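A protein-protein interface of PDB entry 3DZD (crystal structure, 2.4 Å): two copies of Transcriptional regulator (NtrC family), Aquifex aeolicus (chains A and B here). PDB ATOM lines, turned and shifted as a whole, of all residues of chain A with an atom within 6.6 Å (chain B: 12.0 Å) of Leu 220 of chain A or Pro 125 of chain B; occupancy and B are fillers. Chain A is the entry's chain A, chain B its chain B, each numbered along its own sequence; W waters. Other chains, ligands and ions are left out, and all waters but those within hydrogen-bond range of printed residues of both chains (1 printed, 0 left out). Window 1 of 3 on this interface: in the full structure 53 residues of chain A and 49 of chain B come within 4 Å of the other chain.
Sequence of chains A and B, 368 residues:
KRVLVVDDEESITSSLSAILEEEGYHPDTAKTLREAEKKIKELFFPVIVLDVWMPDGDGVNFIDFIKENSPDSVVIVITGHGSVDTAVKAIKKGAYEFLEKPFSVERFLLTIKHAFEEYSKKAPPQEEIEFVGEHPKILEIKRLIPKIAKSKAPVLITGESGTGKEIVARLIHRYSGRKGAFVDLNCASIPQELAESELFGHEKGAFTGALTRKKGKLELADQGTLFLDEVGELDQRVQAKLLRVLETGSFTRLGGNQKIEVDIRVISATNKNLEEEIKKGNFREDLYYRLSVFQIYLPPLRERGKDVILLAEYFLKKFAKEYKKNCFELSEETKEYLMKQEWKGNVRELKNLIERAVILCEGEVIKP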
ATOM      1  N   GLY A 180      21.950  32.613  16.709  1.00  0.00           N
ATOM      2  CA  GLY A 180      20.849  31.680  16.578  1.00  0.00           C
ATOM      3  C   GLY A 180      20.105  31.842  15.264  1.00  0.00           C
ATOM      4  O   GLY A 180      20.427  32.711  14.456  1.00  0.00           O
ATOM      5  N   ALA A 181      19.086  31.010  15.066  1.00  0.00           N
ATOM      6  CA  ALA A 181      18.381  30.936  13.793  1.00  0.00           C
ATOM      7  C   ALA A 181      17.311  32.011  13.630  1.00  0.00           C
ATOM      8  O   ALA A 181      16.869  32.630  14.607  1.00  0.00           O
ATOM      9  CB  ALA A 181      17.759  29.552  13.619  1.00  0.00           C
ATOM     10  N   PHE A 182      16.909  32.219  12.378  1.00  0.00           N
ATOM     11  CA  PHE A 182      15.772  33.070  12.049  1.00  0.00           C
ATOM     12  C   PHE A 182      14.571  32.164  11.875  1.00  0.00           C
ATOM     13  O   PHE A 182      14.479  31.416  10.904  1.00  0.00           O
ATOM     14  CB  PHE A 182      16.026  33.871  10.769  1.00  0.00           C
ATOM     15  CG  PHE A 182      14.899  34.820  10.403  1.00  0.00           C
ATOM     16  CD1 PHE A 182      14.876  36.122  10.901  1.00  0.00           C
ATOM     17  CD2 PHE A 182      13.865  34.410   9.553  1.00  0.00           C
ATOM     18  CE1 PHE A 182      13.844  36.995  10.566  1.00  0.00           C
ATOM     19  CE2 PHE A 182      12.827  35.277   9.216  1.00  0.00           C
ATOM     20  CZ  PHE A 182      12.815  36.571   9.720  1.00  0.00           C
ATOM     21  N   VAL A 183      13.662  32.218  12.836  1.00  0.00           N
ATOM     22  CA  VAL A 183      12.473  31.382  12.826  1.00  0.00           C
ATOM     23  C   VAL A 183      11.264  32.245  12.467  1.00  0.00           C
ATOM     24  O   VAL A 183      10.932  33.182  13.187  1.00  0.00           O
ATOM     25  CB  VAL A 183      12.258  30.753  14.215  1.00  0.00           C
ATOM     26  CG1 VAL A 183      11.011  29.896  14.238  1.00  0.00           C
ATOM     27  CG2 VAL A 183      13.471  29.942  14.612  1.00  0.00           C
ATOM     28  N   GLU A 198       2.542  25.419  17.243  1.00  0.00           N
ATOM     29  CA  GLU A 198       3.711  25.802  16.462  1.00  0.00           C
ATOM     30  C   GLU A 198       4.711  26.551  17.327  1.00  0.00           C
ATOM     31  O   GLU A 198       5.920  26.407  17.165  1.00  0.00           O
ATOM     32  CB  GLU A 198       3.289  26.686  15.288  1.00  0.00           C
ATOM     33  CG  GLU A 198       2.658  25.923  14.160  1.00  0.00           C
ATOM     34  CD  GLU A 198       3.666  25.072  13.430  1.00  0.00           C
ATOM     35  OE1 GLU A 198       4.539  25.651  12.746  1.00  0.00           O
ATOM     36  OE2 GLU A 198       3.586  23.827  13.539  1.00  0.00           O
ATOM     37  N   LEU A 199       4.190  27.355  18.246  1.00  0.00           N
ATOM     38  CA  LEU A 199       5.023  28.189  19.097  1.00  0.00           C
ATOM     39  C   LEU A 199       5.625  27.402  20.253  1.00  0.00           C
ATOM     40  O   LEU A 199       6.829  27.477  20.508  1.00  0.00           O
ATOM     41  CB  LEU A 199       4.203  29.352  19.670  1.00  0.00           C
ATOM     42  CG  LEU A 199       4.091  30.652  18.877  1.00  0.00           C
ATOM     43  CD1 LEU A 199       3.304  31.692  19.673  1.00  0.00           C
ATOM     44  CD2 LEU A 199       5.469  31.184  18.534  1.00  0.00           C
ATOM     45  N   LYS A 214       7.865  17.360  19.847  1.00  0.00           N
ATOM     46  CA  LYS A 214       8.247  18.319  18.814  1.00  0.00           C
ATOM     47  C   LYS A 214       8.558  19.678  19.439  1.00  0.00           C
ATOM     48  O   LYS A 214       7.806  20.174  20.276  1.00  0.00           O
ATOM     49  CB  LYS A 214       7.138  18.466  17.768  1.00  0.00           C
ATOM     50  CG  LYS A 214       7.526  19.329  16.567  1.00  0.00           C
ATOM     51  CD  LYS A 214       6.302  19.921  15.859  1.00  0.00           C
ATOM     52  CE  LYS A 214       5.568  20.942  16.734  1.00  0.00           C
ATOM     53  NZ  LYS A 214       4.358  21.504  16.063  1.00  0.00           N
ATOM     54  N   LYS A 215       9.669  20.277  19.023  1.00  0.00           N
ATOM     55  CA  LYS A 215      10.099  21.566  19.561  1.00  0.00           C
ATOM     56  C   LYS A 215       9.287  22.718  18.966  1.00  0.00           C
ATOM     57  O   LYS A 215       9.028  22.757  17.760  1.00  0.00           O
ATOM     58  CB  LYS A 215      11.586  21.795  19.277  1.00  0.00           C
ATOM     59  CG  LYS A 215      12.440  20.550  19.367  1.00  0.00           C
ATOM     60  CD  LYS A 215      13.898  20.839  19.034  1.00  0.00           C
ATOM     61  CE  LYS A 215      14.671  21.321  20.255  1.00  0.00           C
ATOM     62  NZ  LYS A 215      16.136  21.038  20.149  1.00  0.00           N
ATOM     63  N   GLY A 216       8.893  23.662  19.812  1.00  0.00           N
ATOM     64  CA  GLY A 216       8.191  24.840  19.341  1.00  0.00           C
ATOM     65  C   GLY A 216       9.139  25.849  18.722  1.00  0.00           C
ATOM     66  O   GLY A 216      10.352  25.786  18.936  1.00  0.00           O
ATOM     67  N   LYS A 217       8.582  26.775  17.949  1.00  0.00           N
ATOM     68  CA  LYS A 217       9.358  27.837  17.325  1.00  0.00           C
ATOM     69  C   LYS A 217      10.046  28.705  18.384  1.00  0.00           C
ATOM     70  O   LYS A 217      11.160  29.184  18.177  1.00  0.00           O
ATOM     71  CB  LYS A 217       8.455  28.715  16.454  1.00  0.00           C
ATOM     72  CG  LYS A 217       7.611  27.957  15.456  1.00  0.00           C
ATOM     73  CD  LYS A 217       8.367  27.691  14.163  1.00  0.00           C
ATOM     74  CE  LYS A 217       7.414  27.580  12.975  1.00  0.00           C
ATOM     75  NZ  LYS A 217       8.138  27.427  11.684  1.00  0.00           N
ATOM     76  N   LEU A 218       9.378  28.925  19.510  1.00  0.00           N
ATOM     77  CA  LEU A 218      10.000  29.687  20.591  1.00  0.00           C
ATOM     78  C   LEU A 218      11.394  29.128  20.871  1.00  0.00           C
ATOM     79  O   LEU A 218      12.378  29.861  20.903  1.00  0.00           O
ATOM     80  CB  LEU A 218       9.146  29.641  21.860  1.00  0.00           C
ATOM     81  CG  LEU A 218       7.939  30.575  21.895  1.00  0.00           C
ATOM     82  CD1 LEU A 218       6.905  30.115  22.913  1.00  0.00           C
ATOM     83  CD2 LEU A 218       8.398  31.985  22.190  1.00  0.00           C
ATOM     84  N   GLU A 219      11.456  27.813  21.033  1.00  0.00           N
ATOM     85  CA  GLU A 219      12.688  27.102  21.334  1.00  0.00           C
ATOM     86  C   GLU A 219      13.677  27.084  20.167  1.00  0.00           C
ATOM     87  O   GLU A 219      14.891  27.146  20.370  1.00  0.00           O
ATOM     88  CB  GLU A 219      12.333  25.673  21.730  1.00  0.00           C
ATOM     89  CG  GLU A 219      13.491  24.822  22.159  1.00  0.00           C
ATOM     90  CD  GLU A 219      13.021  23.485  22.691  1.00  0.00           C
ATOM     91  OE1 GLU A 219      11.787  23.290  22.767  1.00  0.00           O
ATOM     92  OE2 GLU A 219      13.876  22.638  23.032  1.00  0.00           O
ATOM     93  N   LEU A 220      13.157  26.989  18.947  1.00  0.00           N
ATOM     94  CA  LEU A 220      14.009  26.941  17.758  1.00  0.00           C
ATOM     95  C   LEU A 220      14.695  28.281  17.513  1.00  0.00           C
ATOM     96  O   LEU A 220      15.671  28.366  16.767  1.00  0.00           O
ATOM     97  CB  LEU A 220      13.190  26.549  16.527  1.00  0.00           C
ATOM     98  CG  LEU A 220      12.743  25.086  16.452  1.00  0.00           C
ATOM     99  CD1 LEU A 220      11.523  24.930  15.565  1.00  0.00           C
ATOM    100  CD2 LEU A 220      13.874  24.212  15.963  1.00  0.00           C
ATOM    101  N   ALA A 221      14.183  29.328  18.149  1.00  0.00           N
ATOM    102  CA  ALA A 221      14.699  30.673  17.932  1.00  0.00           C
ATOM    103  C   ALA A 221      15.717  31.080  18.992  1.00  0.00           C
ATOM    104  O   ALA A 221      16.210  32.202  18.986  1.00  0.00           O
ATOM    105  CB  ALA A 221      13.556  31.671  17.876  1.00  0.00           C
ATOM    106  N   ASP A 222      16.027  30.157  19.897  1.00  0.00           N
ATOM    107  CA  ASP A 222      17.007  30.399  20.948  1.00  0.00           C
ATOM    108  C   ASP A 222      18.255  31.079  20.399  1.00  0.00           C
ATOM    109  O   ASP A 222      18.856  30.625  19.424  1.00  0.00           O
ATOM    110  CB  ASP A 222      17.383  29.085  21.635  1.00  0.00           C
ATOM    111  CG  ASP A 222      18.001  29.295  23.017  1.00  0.00           C
ATOM    112  OD1 ASP A 222      17.865  30.398  23.597  1.00  0.00           O
ATOM    113  OD2 ASP A 222      18.616  28.339  23.525  1.00  0.00           O
ATOM    114  N   GLN A 223      18.625  32.183  21.035  1.00  0.00           N
ATOM    115  CA  GLN A 223      19.765  33.005  20.622  1.00  0.00           C
ATOM    116  C   GLN A 223      19.645  33.546  19.200  1.00  0.00           C
ATOM    117  O   GLN A 223      20.617  34.037  18.634  1.00  0.00           O
ATOM    118  CB  GLN A 223      21.082  32.252  20.797  1.00  0.00           C
ATOM    119  CG  GLN A 223      21.321  31.768  22.224  1.00  0.00           C
ATOM    120  CD  GLN A 223      22.780  31.438  22.490  1.00  0.00           C
ATOM    121  OE1 GLN A 223      23.621  32.334  22.615  1.00  0.00           O
ATOM    122  NE2 GLN A 223      23.087  30.149  22.580  1.00  0.00           N
ATOM    123  N   GLY A 224      18.446  33.463  18.635  1.00  0.00           N
ATOM    124  CA  GLY A 224      18.177  34.025  17.329  1.00  0.00           C
ATOM    125  C   GLY A 224      17.016  35.005  17.332  1.00  0.00           C
ATOM    126  O   GLY A 224      16.774  35.718  18.305  1.00  0.00           O
ATOM    127  N   LEU A 226      12.895  35.499  16.375  1.00  0.00           N
ATOM    128  CA  LEU A 226      11.598  34.929  16.057  1.00  0.00           C
ATOM    129  C   LEU A 226      10.777  35.997  15.341  1.00  0.00           C
ATOM    130  O   LEU A 226      10.525  37.056  15.909  1.00  0.00           O
ATOM    131  CB  LEU A 226      10.892  34.508  17.347  1.00  0.00           C
ATOM    132  CG  LEU A 226       9.542  33.819  17.204  1.00  0.00           C
ATOM    133  CD1 LEU A 226       9.730  32.404  16.687  1.00  0.00           C
ATOM    134  CD2 LEU A 226       8.808  33.819  18.536  1.00  0.00           C
ATOM    135  N   VAL A 262      14.128  30.691  27.169  1.00  0.00           N
ATOM    136  CA  VAL A 262      14.569  31.096  25.840  1.00  0.00           C
ATOM    137  C   VAL A 262      15.187  32.478  25.809  1.00  0.00           C
ATOM    138  O   VAL A 262      15.010  33.294  26.712  1.00  0.00           O
ATOM    139  CB  VAL A 262      13.451  31.032  24.782  1.00  0.00           C
ATOM    140  CG1 VAL A 262      13.778  29.976  23.724  1.00  0.00           C
ATOM    141  CG2 VAL A 262      12.100  30.788  25.434  1.00  0.00           C
ATOM    142  N   ILE A 264      15.233  35.120  22.856  1.00  0.00           N
ATOM    143  CA  ILE A 264      14.856  35.465  21.497  1.00  0.00           C
ATOM    144  C   ILE A 264      14.700  36.959  21.336  1.00  0.00           C
ATOM    145  O   ILE A 264      14.254  37.650  22.243  1.00  0.00           O
ATOM    146  CB  ILE A 264      13.528  34.811  21.107  1.00  0.00           C
ATOM    147  CG1 ILE A 264      12.474  35.094  22.174  1.00  0.00           C
ATOM    148  CG2 ILE A 264      13.698  33.310  20.926  1.00  0.00           C
ATOM    149  CD1 ILE A 264      11.352  34.085  22.197  1.00  0.00           C
ATOM    150  N   PHE B  44      14.615  22.602  32.340  1.00  0.00           N
ATOM    151  CA  PHE B  44      15.483  22.097  31.292  1.00  0.00           C
ATOM    152  C   PHE B  44      16.917  22.628  31.436  1.00  0.00           C
ATOM    153  O   PHE B  44      17.144  23.838  31.378  1.00  0.00           O
ATOM    154  CB  PHE B  44      14.947  22.435  29.897  1.00  0.00           C
ATOM    155  CG  PHE B  44      15.881  22.022  28.804  1.00  0.00           C
ATOM    156  CD1 PHE B  44      16.090  20.682  28.531  1.00  0.00           C
ATOM    157  CD2 PHE B  44      16.598  22.959  28.098  1.00  0.00           C
ATOM    158  CE1 PHE B  44      16.976  20.295  27.555  1.00  0.00           C
ATOM    159  CE2 PHE B  44      17.485  22.571  27.115  1.00  0.00           C
ATOM    160  CZ  PHE B  44      17.674  21.238  26.849  1.00  0.00           C
ATOM    161  N   PRO B  71      15.612  14.926  26.742  1.00  0.00           N
ATOM    162  CA  PRO B  71      16.281  14.399  25.548  1.00  0.00           C
ATOM    163  C   PRO B  71      17.363  15.312  24.997  1.00  0.00           C
ATOM    164  O   PRO B  71      18.380  14.806  24.543  1.00  0.00           O
ATOM    165  CB  PRO B  71      15.142  14.286  24.527  1.00  0.00           C
ATOM    166  CG  PRO B  71      13.928  14.143  25.335  1.00  0.00           C
ATOM    167  CD  PRO B  71      14.148  14.947  26.582  1.00  0.00           C
ATOM    168  N   ASP B  72      17.146  16.624  25.025  1.00  0.00           N
ATOM    169  CA  ASP B  72      18.105  17.574  24.460  1.00  0.00           C
ATOM    170  C   ASP B  72      19.223  17.982  25.411  1.00  0.00           C
ATOM    171  O   ASP B  72      20.035  18.843  25.078  1.00  0.00           O
ATOM    172  CB  ASP B  72      17.386  18.832  23.975  1.00  0.00           C
ATOM    173  CG  ASP B  72      16.275  18.527  22.992  1.00  0.00           C
ATOM    174  OD1 ASP B  72      16.509  17.737  22.048  1.00  0.00           O
ATOM    175  OD2 ASP B  72      15.170  19.087  23.167  1.00  0.00           O
ATOM    176  N   GLU B 118      27.623  21.574  21.317  1.00  0.00           N
ATOM    177  CA  GLU B 118      26.864  20.394  20.928  1.00  0.00           C
ATOM    178  C   GLU B 118      25.369  20.631  21.081  1.00  0.00           C
ATOM    179  O   GLU B 118      24.568  20.237  20.224  1.00  0.00           O
ATOM    180  CB  GLU B 118      27.293  19.176  21.738  1.00  0.00           C
ATOM    181  CG  GLU B 118      26.604  17.893  21.323  1.00  0.00           C
ATOM    182  CD  GLU B 118      27.041  17.405  19.948  1.00  0.00           C
ATOM    183  OE1 GLU B 118      27.916  18.047  19.327  1.00  0.00           O
ATOM    184  OE2 GLU B 118      26.513  16.370  19.488  1.00  0.00           O
ATOM    185  N   TYR B 119      24.996  21.280  22.173  1.00  0.00           N
ATOM    186  CA  TYR B 119      23.605  21.604  22.418  1.00  0.00           C
ATOM    187  C   TYR B 119      23.067  22.516  21.321  1.00  0.00           C
ATOM    188  O   TYR B 119      21.977  22.298  20.791  1.00  0.00           O
ATOM    189  CB  TYR B 119      23.444  22.277  23.782  1.00  0.00           C
ATOM    190  CG  TYR B 119      22.139  23.014  23.916  1.00  0.00           C
ATOM    191  CD1 TYR B 119      20.936  22.324  23.994  1.00  0.00           C
ATOM    192  CD2 TYR B 119      22.106  24.400  23.952  1.00  0.00           C
ATOM    193  CE1 TYR B 119      19.738  22.994  24.110  1.00  0.00           C
ATOM    194  CE2 TYR B 119      20.918  25.077  24.070  1.00  0.00           C
ATOM    195  CZ  TYR B 119      19.735  24.371  24.148  1.00  0.00           C
ATOM    196  OH  TYR B 119      18.546  25.052  24.262  1.00  0.00           O
ATOM    197  N   SER B 120      23.847  23.530  20.976  1.00  0.00           N
ATOM    198  CA  SER B 120      23.401  24.546  20.036  1.00  0.00           C
ATOM    199  C   SER B 120      23.470  24.122  18.567  1.00  0.00           C
ATOM    200  O   SER B 120      22.823  24.729  17.719  1.00  0.00           O
ATOM    201  CB  SER B 120      24.195  25.832  20.240  1.00  0.00           C
ATOM    202  OG  SER B 120      23.827  26.454  21.457  1.00  0.00           O
ATOM    203  N   LYS B 121      24.264  23.103  18.264  1.00  0.00           N
ATOM    204  CA  LYS B 121      24.396  22.640  16.888  1.00  0.00           C
ATOM    205  C   LYS B 121      23.249  21.711  16.531  1.00  0.00           C
ATOM    206  O   LYS B 121      23.284  20.519  16.833  1.00  0.00           O
ATOM    207  CB  LYS B 121      25.733  21.929  16.668  1.00  0.00           C
ATOM    208  CG  LYS B 121      26.938  22.857  16.542  1.00  0.00           C
ATOM    209  CD  LYS B 121      28.235  22.056  16.432  1.00  0.00           C
ATOM    210  CE  LYS B 121      29.446  22.962  16.278  1.00  0.00           C
ATOM    211  NZ  LYS B 121      30.720  22.204  16.418  1.00  0.00           N
ATOM    212  N   LYS B 122      22.229  22.262  15.886  1.00  0.00           N
ATOM    213  CA  LYS B 122      21.058  21.480  15.529  1.00  0.00           C
ATOM    214  C   LYS B 122      20.562  21.815  14.131  1.00  0.00           C
ATOM    215  O   LYS B 122      20.694  22.946  13.666  1.00  0.00           O
ATOM    216  CB  LYS B 122      19.941  21.699  16.548  1.00  0.00           C
ATOM    217  CG  LYS B 122      20.120  20.912  17.834  1.00  0.00           C
ATOM    218  CD  LYS B 122      20.016  19.422  17.570  1.00  0.00           C
ATOM    219  CE  LYS B 122      19.904  18.641  18.866  1.00  0.00           C
ATOM    220  NZ  LYS B 122      19.556  17.213  18.619  1.00  0.00           N
ATOM    221  N   ALA B 123      19.996  20.817  13.467  1.00  0.00           N
ATOM    222  CA  ALA B 123      19.396  21.019  12.159  1.00  0.00           C
ATOM    223  C   ALA B 123      17.910  21.296  12.335  1.00  0.00           C
ATOM    224  O   ALA B 123      17.276  20.720  13.217  1.00  0.00           O
ATOM    225  CB  ALA B 123      19.609  19.795  11.285  1.00  0.00           C
ATOM    226  N   PRO B 124      17.356  22.189  11.500  1.00  0.00           N
ATOM    227  CA  PRO B 124      15.931  22.535  11.519  1.00  0.00           C
ATOM    228  C   PRO B 124      15.059  21.309  11.271  1.00  0.00           C
ATOM    229  O   PRO B 124      14.839  20.943  10.116  1.00  0.00           O
ATOM    230  CB  PRO B 124      15.792  23.512  10.348  1.00  0.00           C
ATOM    231  CG  PRO B 124      17.162  24.068  10.153  1.00  0.00           C
ATOM    232  CD  PRO B 124      18.100  22.953  10.485  1.00  0.00           C
ATOM    233  N   PRO B 125      14.557  20.688  12.349  1.00  0.00           N
ATOM    234  CA  PRO B 125      13.813  19.430  12.244  1.00  0.00           C
ATOM    235  C   PRO B 125      12.654  19.539  11.263  1.00  0.00           C
ATOM    236  O   PRO B 125      12.328  18.559  10.593  1.00  0.00           O
ATOM    237  CB  PRO B 125      13.286  19.216  13.666  1.00  0.00           C
ATOM    238  CG  PRO B 125      14.210  19.998  14.536  1.00  0.00           C
ATOM    239  CD  PRO B 125      14.571  21.204  13.728  1.00  0.00           C
ATOM    240  N   GLN B 126      12.043  20.717  11.179  1.00  0.00           N
ATOM    241  CA  GLN B 126      10.938  20.917  10.251  1.00  0.00           C
ATOM    242  C   GLN B 126      11.436  20.799   8.819  1.00  0.00           C
ATOM    243  O   GLN B 126      12.453  21.389   8.451  1.00  0.00           O
ATOM    244  CB  GLN B 126      10.253  22.269  10.472  1.00  0.00           C
ATOM    245  CG  GLN B 126      11.048  23.471   9.998  1.00  0.00           C
ATOM    246  CD  GLN B 126      10.152  24.624   9.591  1.00  0.00           C
ATOM    247  OE1 GLN B 126      10.474  25.789   9.820  1.00  0.00           O
ATOM    248  NE2 GLN B 126       9.016  24.301   8.983  1.00  0.00           N
ATOM    249  N   GLU B 127      10.715  20.025   8.018  1.00  0.00           N
ATOM    250  CA  GLU B 127      11.136  19.743   6.657  1.00  0.00           C
ATOM    251  C   GLU B 127      10.120  18.865   5.940  1.00  0.00           C
ATOM    252  O   GLU B 127      10.085  17.650   6.132  1.00  0.00           O
ATOM    253  CB  GLU B 127      12.501  19.056   6.668  1.00  0.00           C
ATOM    254  CG  GLU B 127      12.591  17.889   7.639  1.00  0.00           C
ATOM    255  CD  GLU B 127      13.930  17.182   7.584  1.00  0.00           C
ATOM    256  OE1 GLU B 127      14.857  17.706   6.930  1.00  0.00           O
ATOM    257  OE2 GLU B 127      14.056  16.101   8.197  1.00  0.00           O
ATOM    258  N   GLU B 128       9.283  19.487   5.119  1.00  0.00           N
ATOM    259  CA  GLU B 128       8.360  18.737   4.282  1.00  0.00           C
ATOM    260  C   GLU B 128       8.475  19.157   2.833  1.00  0.00           C
ATOM    261  O   GLU B 128       8.371  20.339   2.501  1.00  0.00           O
ATOM    262  CB  GLU B 128       6.918  18.894   4.754  1.00  0.00           C
ATOM    263  CG  GLU B 128       6.439  17.761   5.638  1.00  0.00           C
ATOM    264  CD  GLU B 128       4.992  17.392   5.367  1.00  0.00           C
ATOM    265  OE1 GLU B 128       4.473  17.760   4.289  1.00  0.00           O
ATOM    266  OE2 GLU B 128       4.375  16.728   6.228  1.00  0.00           O
ATOM    267  N   ILE B 129       8.702  18.177   1.972  1.00  0.00           N
ATOM    268  CA  ILE B 129       8.773  18.437   0.543  1.00  0.00           C
ATOM    269  C   ILE B 129       7.508  17.920  -0.128  1.00  0.00           C
ATOM    270  O   ILE B 129       7.178  16.739  -0.033  1.00  0.00           O
ATOM    271  CB  ILE B 129      10.031  17.812  -0.088  1.00  0.00           C
ATOM    272  CG1 ILE B 129      11.247  18.056   0.812  1.00  0.00           C
ATOM    273  CG2 ILE B 129      10.281  18.406  -1.459  1.00  0.00           C
ATOM    274  CD1 ILE B 129      12.567  17.543   0.249  1.00  0.00           C
ATOM    275  N   ARG B 174      17.028  13.583   0.590  1.00  0.00           N
ATOM    276  CA  ARG B 174      16.317  13.312   1.828  1.00  0.00           C
ATOM    277  C   ARG B 174      16.328  11.816   2.133  1.00  0.00           C
ATOM    278  O   ARG B 174      16.872  11.386   3.149  1.00  0.00           O
ATOM    279  CB  ARG B 174      14.890  13.863   1.743  1.00  0.00           C
ATOM    280  CG  ARG B 174      13.913  13.349   2.791  1.00  0.00           C
ATOM    281  CD  ARG B 174      14.029  14.084   4.119  1.00  0.00           C
ATOM    282  NE  ARG B 174      13.925  15.541   3.998  1.00  0.00           N
ATOM    283  CZ  ARG B 174      12.779  16.216   3.913  1.00  0.00           C
ATOM    284  NH1 ARG B 174      11.617  15.568   3.911  1.00  0.00           N
ATOM    285  NH2 ARG B 174      12.797  17.542   3.817  1.00  0.00           N
ATOM    286  N   LYS B 179      24.272  13.202   5.380  1.00  0.00           N
ATOM    287  CA  LYS B 179      24.229  14.205   6.436  1.00  0.00           C
ATOM    288  C   LYS B 179      24.680  15.594   5.993  1.00  0.00           C
ATOM    289  O   LYS B 179      24.328  16.587   6.616  1.00  0.00           O
ATOM    290  CB  LYS B 179      25.064  13.746   7.636  1.00  0.00           C
ATOM    291  CG  LYS B 179      24.658  12.391   8.198  1.00  0.00           C
ATOM    292  CD  LYS B 179      23.250  12.420   8.781  1.00  0.00           C
ATOM    293  CE  LYS B 179      23.197  13.207  10.081  1.00  0.00           C
ATOM    294  NZ  LYS B 179      21.904  13.005  10.792  1.00  0.00           N
HETATM  295  O   HOH W   1      14.201  20.643  25.661  1.00  0.00           O
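Water W1 bridges OD2 of Asp 72 of chain B (3.1 Å) and OE2 of Glu 219 of chain A (3.3 Å).
No position is printed for both chains.
Among the printed residues, merely in contact across the chains: Glu 219 of chain A with Asp 72 of chain B, Leu 220 of chain A with Pro 125 of chain B and Gln 223 of chain A with Ser 120 of chain B.
Printed residues of chain A that touch a printed residue of chain B: Lys 215, Lys 217, Glu 219, Leu 220, Asp 222 and Gln 223. Hydrophobic or aromatic side chains of chain B within 4 Å of the printed part of chain A: Tyr 119 and Pro 125. Among the printed residues, Asp or Glu carboxylates within 4 Å of a Lys or Arg side-chain nitrogen of the other chain: Lys 215 of chain A with Asp 72 of chain B (3.7 Å).
Leu 220 of chain A touches one residue of chain B. Pro 125 of chain B touches just one residue of chain A: Leu 220. No residue of chain B comes within 4 Å of Gly 180 of chain A. No residue of chain B comes within 4 Å of Ala 181 of chain A. No residue of chain B comes within 4 Å of Gly 216 of chain A. Of chain B, only Gln 126 comes within 4 Å of Lys 217 of chain A. Of chain B, only Asp 72 (3.8 Å) comes within 4 Å of Glu 219 of chain A. No residue of chain B comes within 4 Å of Ala 221 of chain A. Asp 222 of chain A touches one residue of chain B. Gly 224 of chain A touches none of the printed residues of chain B. Of the printed residues of chain A, Ser 120 of chain B touches Gln 223. Of the printed residues of chain B, Gln 223 of chain A touches Ser 120. Of the printed residues of chain A, Asp 72 of chain B touches Lys 215 and Glu 219. Printed residues of chain A within 4 Å of Tyr 119 of chain B: Asp 222. The nearest residue of chain A that does not touch Pro 125 of chain B is Lys 215 of chain A (4.6 Å). The nearest printed residue of chain A that does not touch Ser 120 of chain B is Asp 222 of chain A (5.9 Å).
The backbone NH (N) of Gly 180 of chain A sits at hydrogen-bond distance from the backbone carbonyl oxygen (O) of Gln 223 of chain A, 2.7 Å away. The backbone carbonyl oxygen of Glu 198 of chain A is in hydrogen-bond range of the backbone NH of Lys 217 of chain A. The backbone NH (N) of Lys 217 of chain A sits at hydrogen-bond distance from the backbone carbonyl oxygen (O) of Leu 199 of chain A, at 3.2 Å. NZ of Lys 215 of chain A is in salt-bridge range of OE2 of Glu 219 of chain A, 3.997 Å away.
NZ of Lys 215 of chain A lies within salt-bridge range of OD2 of Asp 72 of chain B, at 3.7 Å. NZ of Lys 217 of chain A is in hydrogen-bond range of OE1 of Gln 126 of chain B (3.4 Å). The side-chain carboxylate of Asp 222 of chain A is in hydrogen-bond range of the side-chain hydroxyl of Tyr 119 of chain B, at 3.4 Å.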
